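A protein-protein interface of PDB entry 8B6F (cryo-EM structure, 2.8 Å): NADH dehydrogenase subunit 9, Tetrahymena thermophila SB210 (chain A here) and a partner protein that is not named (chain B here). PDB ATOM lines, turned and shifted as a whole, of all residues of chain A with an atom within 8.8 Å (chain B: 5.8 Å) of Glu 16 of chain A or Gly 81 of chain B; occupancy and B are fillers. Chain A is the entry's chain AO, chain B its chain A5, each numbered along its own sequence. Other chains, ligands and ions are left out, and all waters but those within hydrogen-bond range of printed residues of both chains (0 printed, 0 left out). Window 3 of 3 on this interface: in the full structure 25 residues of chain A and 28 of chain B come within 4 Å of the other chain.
Of chain B, only Pro 79, Val 80, Gly 81 and Lys 138 come within 4 Å of Glu 16 of chain A. Of the printed residues of chain A, Gly 81 of chain B touches Glu 16. Val 80 of chain B touches just these residues of chain A: Phe 12 (3.4 Å), Ile 13 (3.8 Å) and Glu 16 (3.5 Å). Printed residues of chain B within 4 Å of Ile 13 of chain A: Val 80. Of the printed residues of chain B, Phe 12 of chain A touches Val 80. Of the printed residues of chain A, Lys 138 of chain B touches Glu 16. Of the printed residues of chain B, Leu 18 of chain A touches Pro 79. Printed residues of chain A within 4 Å of Pro 79 of chain B: Glu 16 and Leu 18. Glu 139 of chain B touches none of the printed residues of chain A. The nearest printed residue of chain A that does not touch Pro 79 of chain B is Asn 19 of chain A (4.1 Å).
Of the 13 printed residues of chain A, 4 touch a printed residue of chain B. Along chain A the printed residues that touch a printed residue of chain B span positions 12 to 18. Among the printed residues, 7 pairs touch across the chains. Among the printed residues, no Asp or Glu carboxylate lies within 4 Å of a Lys or Arg side-chain nitrogen of the other chain.
O of Phe 12 of chain A touches CG2 of Val 80 of chain B (3.4 Å). Ile 13 of chain A touches Val 80 of chain B. Pro 79 of chain B touches Glu 16 of chain A (CB to O, 3.4 Å). Val 80 of chain B touches Glu 16 of chain A (CG2 to CA, 3.5 Å). Glu 16 of chain A touches Lys 138 of chain B. CA of Pro 79 of chain B touches O of Leu 18 of chain A, 3.4 Å away.
O of Glu 16 of chain A lies within hydrogen-bond range of N of Gly 81 of chain B (2.7 Å).
O of Val 80 of chain B lies close to N of Lys 138 of chain B (3.5 Å).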
ATOM      1  N   ILE A   9      -2.202  -3.145 -21.919  1.00  0.00           N
ATOM      2  CA  ILE A   9      -1.057  -4.018 -21.667  1.00  0.00           C
ATOM      3  C   ILE A   9      -0.689  -4.085 -20.195  1.00  0.00           C
ATOM      4  O   ILE A   9       0.225  -4.832 -19.827  1.00  0.00           O
ATOM      5  CB  ILE A   9       0.141  -3.542 -22.517  1.00  0.00           C
ATOM      6  CG1 ILE A   9       1.217  -4.629 -22.628  1.00  0.00           C
ATOM      7  CG2 ILE A   9       0.739  -2.266 -21.946  1.00  0.00           C
ATOM      8  CD1 ILE A   9       0.779  -5.867 -23.385  1.00  0.00           C
ATOM      9  N   GLN A  10      -1.380  -3.334 -19.335  1.00  0.00           N
ATOM     10  CA  GLN A  10      -1.076  -3.377 -17.908  1.00  0.00           C
ATOM     11  C   GLN A  10      -1.319  -4.766 -17.338  1.00  0.00           C
ATOM     12  O   GLN A  10      -0.533  -5.258 -16.520  1.00  0.00           O
ATOM     13  CB  GLN A  10      -1.916  -2.346 -17.155  1.00  0.00           C
ATOM     14  CG  GLN A  10      -1.598  -0.903 -17.487  1.00  0.00           C
ATOM     15  CD  GLN A  10      -2.120  -0.481 -18.845  1.00  0.00           C
ATOM     16  OE1 GLN A  10      -2.982  -1.137 -19.421  1.00  0.00           O
ATOM     17  NE2 GLN A  10      -1.589   0.620 -19.365  1.00  0.00           N
ATOM     18  N   LEU A  11      -2.406  -5.416 -17.758  1.00  0.00           N
ATOM     19  CA  LEU A  11      -2.720  -6.745 -17.249  1.00  0.00           C
ATOM     20  C   LEU A  11      -1.573  -7.712 -17.490  1.00  0.00           C
ATOM     21  O   LEU A  11      -1.156  -8.441 -16.585  1.00  0.00           O
ATOM     22  CB  LEU A  11      -3.997  -7.269 -17.903  1.00  0.00           C
ATOM     23  CG  LEU A  11      -5.319  -6.685 -17.410  1.00  0.00           C
ATOM     24  CD1 LEU A  11      -6.471  -7.210 -18.254  1.00  0.00           C
ATOM     25  CD2 LEU A  11      -5.522  -7.007 -15.940  1.00  0.00           C
ATOM     26  N   PHE A  12      -1.047  -7.730 -18.710  1.00  0.00           N
ATOM     27  CA  PHE A  12       0.007  -8.672 -19.056  1.00  0.00           C
ATOM     28  C   PHE A  12       1.375  -8.227 -18.556  1.00  0.00           C
ATOM     29  O   PHE A  12       2.273  -9.066 -18.429  1.00  0.00           O
ATOM     30  CB  PHE A  12       0.026  -8.877 -20.569  1.00  0.00           C
ATOM     31  CG  PHE A  12      -1.324  -9.201 -21.141  1.00  0.00           C
ATOM     32  CD1 PHE A  12      -1.803 -10.500 -21.122  1.00  0.00           C
ATOM     33  CD2 PHE A  12      -2.119  -8.206 -21.682  1.00  0.00           C
ATOM     34  CE1 PHE A  12      -3.046 -10.801 -21.640  1.00  0.00           C
ATOM     35  CE2 PHE A  12      -3.364  -8.500 -22.202  1.00  0.00           C
ATOM     36  CZ  PHE A  12      -3.828  -9.800 -22.182  1.00  0.00           C
ATOM     37  N   ILE A  13       1.558  -6.937 -18.275  1.00  0.00           N
ATOM     38  CA  ILE A  13       2.783  -6.501 -17.611  1.00  0.00           C
ATOM     39  C   ILE A  13       2.800  -6.978 -16.165  1.00  0.00           C
ATOM     40  O   ILE A  13       3.847  -7.373 -15.640  1.00  0.00           O
ATOM     41  CB  ILE A  13       2.921  -4.968 -17.708  1.00  0.00           C
ATOM     42  CG1 ILE A  13       3.329  -4.566 -19.127  1.00  0.00           C
ATOM     43  CG2 ILE A  13       3.936  -4.441 -16.687  1.00  0.00           C
ATOM     44  CD1 ILE A  13       3.311  -3.074 -19.378  1.00  0.00           C
ATOM     45  N   VAL A  14       1.649  -6.942 -15.497  1.00  0.00           N
ATOM     46  CA  VAL A  14       1.583  -7.357 -14.099  1.00  0.00           C
ATOM     47  C   VAL A  14       1.609  -8.874 -13.987  1.00  0.00           C
ATOM     48  O   VAL A  14       2.395  -9.441 -13.221  1.00  0.00           O
ATOM     49  CB  VAL A  14       0.335  -6.755 -13.430  1.00  0.00           C
ATOM     50  CG1 VAL A  14       0.088  -7.381 -12.064  1.00  0.00           C
ATOM     51  CG2 VAL A  14       0.494  -5.256 -13.306  1.00  0.00           C
ATOM     52  N   PHE A  15       0.749  -9.555 -14.743  1.00  0.00           N
ATOM     53  CA  PHE A  15       0.722 -11.016 -14.760  1.00  0.00           C
ATOM     54  C   PHE A  15       1.775 -11.484 -15.759  1.00  0.00           C
ATOM     55  O   PHE A  15       1.499 -11.790 -16.921  1.00  0.00           O
ATOM     56  CB  PHE A  15      -0.673 -11.521 -15.101  1.00  0.00           C
ATOM     57  CG  PHE A  15      -1.706 -11.173 -14.069  1.00  0.00           C
ATOM     58  CD1 PHE A  15      -2.337  -9.942 -14.083  1.00  0.00           C
ATOM     59  CD2 PHE A  15      -2.037 -12.076 -13.075  1.00  0.00           C
ATOM     60  CE1 PHE A  15      -3.281  -9.620 -13.128  1.00  0.00           C
ATOM     61  CE2 PHE A  15      -2.978 -11.761 -12.116  1.00  0.00           C
ATOM     62  CZ  PHE A  15      -3.602 -10.531 -12.143  1.00  0.00           C
ATOM     63  N   GLU A  16       3.015 -11.543 -15.276  1.00  0.00           N
ATOM     64  CA  GLU A  16       4.175 -11.737 -16.137  1.00  0.00           C
ATOM     65  C   GLU A  16       4.276 -13.138 -16.725  1.00  0.00           C
ATOM     66  O   GLU A  16       5.116 -13.356 -17.602  1.00  0.00           O
ATOM     67  CB  GLU A  16       5.451 -11.420 -15.357  1.00  0.00           C
ATOM     68  CG  GLU A  16       5.638 -12.269 -14.106  1.00  0.00           C
ATOM     69  CD  GLU A  16       6.857 -11.865 -13.306  1.00  0.00           C
ATOM     70  OE1 GLU A  16       7.691 -11.105 -13.838  1.00  0.00           O
ATOM     71  OE2 GLU A  16       6.982 -12.304 -12.145  1.00  0.00           O
ATOM     72  N   LYS A  17       3.461 -14.088 -16.271  1.00  0.00           N
ATOM     73  CA  LYS A  17       3.539 -15.464 -16.741  1.00  0.00           C
ATOM     74  C   LYS A  17       2.534 -15.773 -17.843  1.00  0.00           C
ATOM     75  O   LYS A  17       2.436 -16.929 -18.267  1.00  0.00           O
ATOM     76  CB  LYS A  17       3.337 -16.424 -15.566  1.00  0.00           C
ATOM     77  CG  LYS A  17       4.356 -16.258 -14.445  1.00  0.00           C
ATOM     78  CD  LYS A  17       5.774 -16.527 -14.932  1.00  0.00           C
ATOM     79  CE  LYS A  17       6.780 -16.406 -13.801  1.00  0.00           C
ATOM     80  NZ  LYS A  17       8.178 -16.586 -14.285  1.00  0.00           N
ATOM     81  N   LEU A  18       1.798 -14.775 -18.322  1.00  0.00           N
ATOM     82  CA  LEU A  18       0.778 -14.962 -19.342  1.00  0.00           C
ATOM     83  C   LEU A  18       1.220 -14.349 -20.664  1.00  0.00           C
ATOM     84  O   LEU A  18       1.923 -13.337 -20.697  1.00  0.00           O
ATOM     85  CB  LEU A  18      -0.554 -14.340 -18.911  1.00  0.00           C
ATOM     86  CG  LEU A  18      -1.353 -15.077 -17.835  1.00  0.00           C
ATOM     87  CD1 LEU A  18      -0.586 -15.172 -16.531  1.00  0.00           C
ATOM     88  CD2 LEU A  18      -2.689 -14.393 -17.609  1.00  0.00           C
ATOM     89  N   ASN A  19       0.796 -14.981 -21.753  1.00  0.00           N
ATOM     90  CA  ASN A  19       1.025 -14.464 -23.091  1.00  0.00           C
ATOM     91  C   ASN A  19      -0.179 -13.653 -23.551  1.00  0.00           C
ATOM     92  O   ASN A  19      -1.323 -13.943 -23.190  1.00  0.00           O
ATOM     93  CB  ASN A  19       1.298 -15.604 -24.071  1.00  0.00           C
ATOM     94  CG  ASN A  19       0.175 -16.614 -24.115  1.00  0.00           C
ATOM     95  OD1 ASN A  19       0.168 -17.584 -23.357  1.00  0.00           O
ATOM     96  ND2 ASN A  19      -0.784 -16.395 -25.006  1.00  0.00           N
ATOM     97  N   SER A  20       0.090 -12.629 -24.351  1.00  0.00           N
ATOM     98  CA  SER A  20      -0.917 -11.660 -24.762  1.00  0.00           C
ATOM     99  C   SER A  20      -1.443 -12.008 -26.148  1.00  0.00           C
ATOM    100  O   SER A  20      -0.663 -12.300 -27.059  1.00  0.00           O
ATOM    101  CB  SER A  20      -0.337 -10.247 -24.767  1.00  0.00           C
ATOM    102  OG  SER A  20       0.275  -9.944 -23.528  1.00  0.00           O
ATOM    103  N   TRP A  41      -6.356 -18.007 -14.444  1.00  0.00           N
ATOM    104  CA  TRP A  41      -5.949 -16.672 -14.030  1.00  0.00           C
ATOM    105  C   TRP A  41      -7.093 -15.669 -14.069  1.00  0.00           C
ATOM    106  O   TRP A  41      -6.893 -14.510 -13.698  1.00  0.00           O
ATOM    107  CB  TRP A  41      -4.809 -16.166 -14.920  1.00  0.00           C
ATOM    108  CG  TRP A  41      -3.532 -16.922 -14.772  1.00  0.00           C
ATOM    109  CD1 TRP A  41      -3.114 -17.980 -15.520  1.00  0.00           C
ATOM    110  CD2 TRP A  41      -2.497 -16.668 -13.820  1.00  0.00           C
ATOM    111  NE1 TRP A  41      -1.880 -18.403 -15.092  1.00  0.00           N
ATOM    112  CE2 TRP A  41      -1.480 -17.613 -14.047  1.00  0.00           C
ATOM    113  CE3 TRP A  41      -2.331 -15.731 -12.796  1.00  0.00           C
ATOM    114  CZ2 TRP A  41      -0.313 -17.650 -13.288  1.00  0.00           C
ATOM    115  CZ3 TRP A  41      -1.176 -15.769 -12.044  1.00  0.00           C
ATOM    116  CH2 TRP A  41      -0.179 -16.722 -12.293  1.00  0.00           C
ATOM    117  N   PRO B  79       5.258 -13.844 -22.912  1.00  0.00           N
ATOM    118  CA  PRO B  79       5.218 -13.434 -21.507  1.00  0.00           C
ATOM    119  C   PRO B  79       6.386 -12.520 -21.175  1.00  0.00           C
ATOM    120  O   PRO B  79       7.522 -12.755 -21.591  1.00  0.00           O
ATOM    121  CB  PRO B  79       5.302 -14.762 -20.745  1.00  0.00           C
ATOM    122  CG  PRO B  79       4.846 -15.792 -21.717  1.00  0.00           C
ATOM    123  CD  PRO B  79       5.277 -15.309 -23.063  1.00  0.00           C
ATOM    124  N   VAL B  80       6.095 -11.462 -20.416  1.00  0.00           N
ATOM    125  CA  VAL B  80       7.151 -10.549 -19.999  1.00  0.00           C
ATOM    126  C   VAL B  80       8.031 -11.183 -18.934  1.00  0.00           C
ATOM    127  O   VAL B  80       9.183 -10.769 -18.760  1.00  0.00           O
ATOM    128  CB  VAL B  80       6.558  -9.217 -19.498  1.00  0.00           C
ATOM    129  CG1 VAL B  80       5.798  -8.524 -20.614  1.00  0.00           C
ATOM    130  CG2 VAL B  80       5.655  -9.441 -18.304  1.00  0.00           C
ATOM    131  N   GLY B  81       7.517 -12.176 -18.208  1.00  0.00           N
ATOM    132  CA  GLY B  81       8.326 -12.846 -17.207  1.00  0.00           C
ATOM    133  C   GLY B  81       9.474 -13.639 -17.796  1.00  0.00           C
ATOM    134  O   GLY B  81      10.547 -13.720 -17.192  1.00  0.00           O
ATOM    135  N   GLU B  82       9.272 -14.235 -18.968  1.00  0.00           N
ATOM    136  CA  GLU B  82      10.310 -15.060 -19.571  1.00  0.00           C
ATOM    137  C   GLU B  82      11.561 -14.240 -19.856  1.00  0.00           C
ATOM    138  O   GLU B  82      11.487 -13.084 -20.283  1.00  0.00           O
ATOM    139  CB  GLU B  82       9.800 -15.692 -20.866  1.00  0.00           C
ATOM    140  CG  GLU B  82       8.783 -16.797 -20.652  1.00  0.00           C
ATOM    141  CD  GLU B  82       8.391 -17.481 -21.946  1.00  0.00           C
ATOM    142  OE1 GLU B  82       8.771 -16.978 -23.022  1.00  0.00           O
ATOM    143  OE2 GLU B  82       7.704 -18.523 -21.887  1.00  0.00           O
ATOM    144  N   THR B  83      12.715 -14.849 -19.615  1.00  0.00           N
ATOM    145  CA  THR B  83      13.998 -14.261 -19.962  1.00  0.00           C
ATOM    146  C   THR B  83      14.367 -14.658 -21.390  1.00  0.00           C
ATOM    147  O   THR B  83      13.695 -15.468 -22.031  1.00  0.00           O
ATOM    148  CB  THR B  83      15.068 -14.723 -18.963  1.00  0.00           C
ATOM    149  OG1 THR B  83      14.542 -14.654 -17.633  1.00  0.00           O
ATOM    150  CG2 THR B  83      16.329 -13.858 -19.028  1.00  0.00           C
ATOM    151  N   GLU B  86      15.077 -18.396 -21.424  1.00  0.00           N
ATOM    152  CA  GLU B  86      13.852 -19.184 -21.385  1.00  0.00           C
ATOM    153  C   GLU B  86      13.120 -19.127 -22.718  1.00  0.00           C
ATOM    154  O   GLU B  86      12.590 -20.140 -23.189  1.00  0.00           O
ATOM    155  CB  GLU B  86      12.948 -18.694 -20.255  1.00  0.00           C
ATOM    156  CG  GLU B  86      13.582 -18.798 -18.877  1.00  0.00           C
ATOM    157  CD  GLU B  86      12.640 -18.375 -17.770  1.00  0.00           C
ATOM    158  OE1 GLU B  86      11.458 -18.106 -18.066  1.00  0.00           O
ATOM    159  OE2 GLU B  86      13.080 -18.312 -16.602  1.00  0.00           O
ATOM    160  N   LYS B 138      10.961  -7.797 -18.453  1.00  0.00           N
ATOM    161  CA  LYS B 138      11.354  -7.803 -17.048  1.00  0.00           C
ATOM    162  C   LYS B 138      12.783  -7.311 -16.860  1.00  0.00           C
ATOM    163  O   LYS B 138      13.093  -6.688 -15.838  1.00  0.00           O
ATOM    164  CB  LYS B 138      11.195  -9.211 -16.477  1.00  0.00           C
ATOM    165  CG  LYS B 138      11.558  -9.340 -15.007  1.00  0.00           C
ATOM    166  CD  LYS B 138      11.308 -10.754 -14.507  1.00  0.00           C
ATOM    167  CE  LYS B 138      11.620 -10.880 -13.025  1.00  0.00           C
ATOM    168  NZ  LYS B 138      11.329 -12.247 -12.508  1.00  0.00           N
ATOM    169  N   GLU B 139      13.666  -7.578 -17.824  1.00  0.00           N
ATOM    170  CA  GLU B 139      15.075  -7.236 -17.655  1.00  0.00           C
ATOM    171  C   GLU B 139      15.287  -5.728 -17.695  1.00  0.00           C
ATOM    172  O   GLU B 139      15.989  -5.168 -16.845  1.00  0.00           O
ATOM    173  CB  GLU B 139      15.915  -7.925 -18.731  1.00  0.00           C
ATOM    174  CG  GLU B 139      15.970  -9.441 -18.605  1.00  0.00           C
ATOM    175  CD  GLU B 139      14.659 -10.108 -18.972  1.00  0.00           C
ATOM    176  OE1 GLU B 139      13.844  -9.476 -19.675  1.00  0.00           O
ATOM    177  OE2 GLU B 139      14.438 -11.263 -18.553  1.00  0.00           O
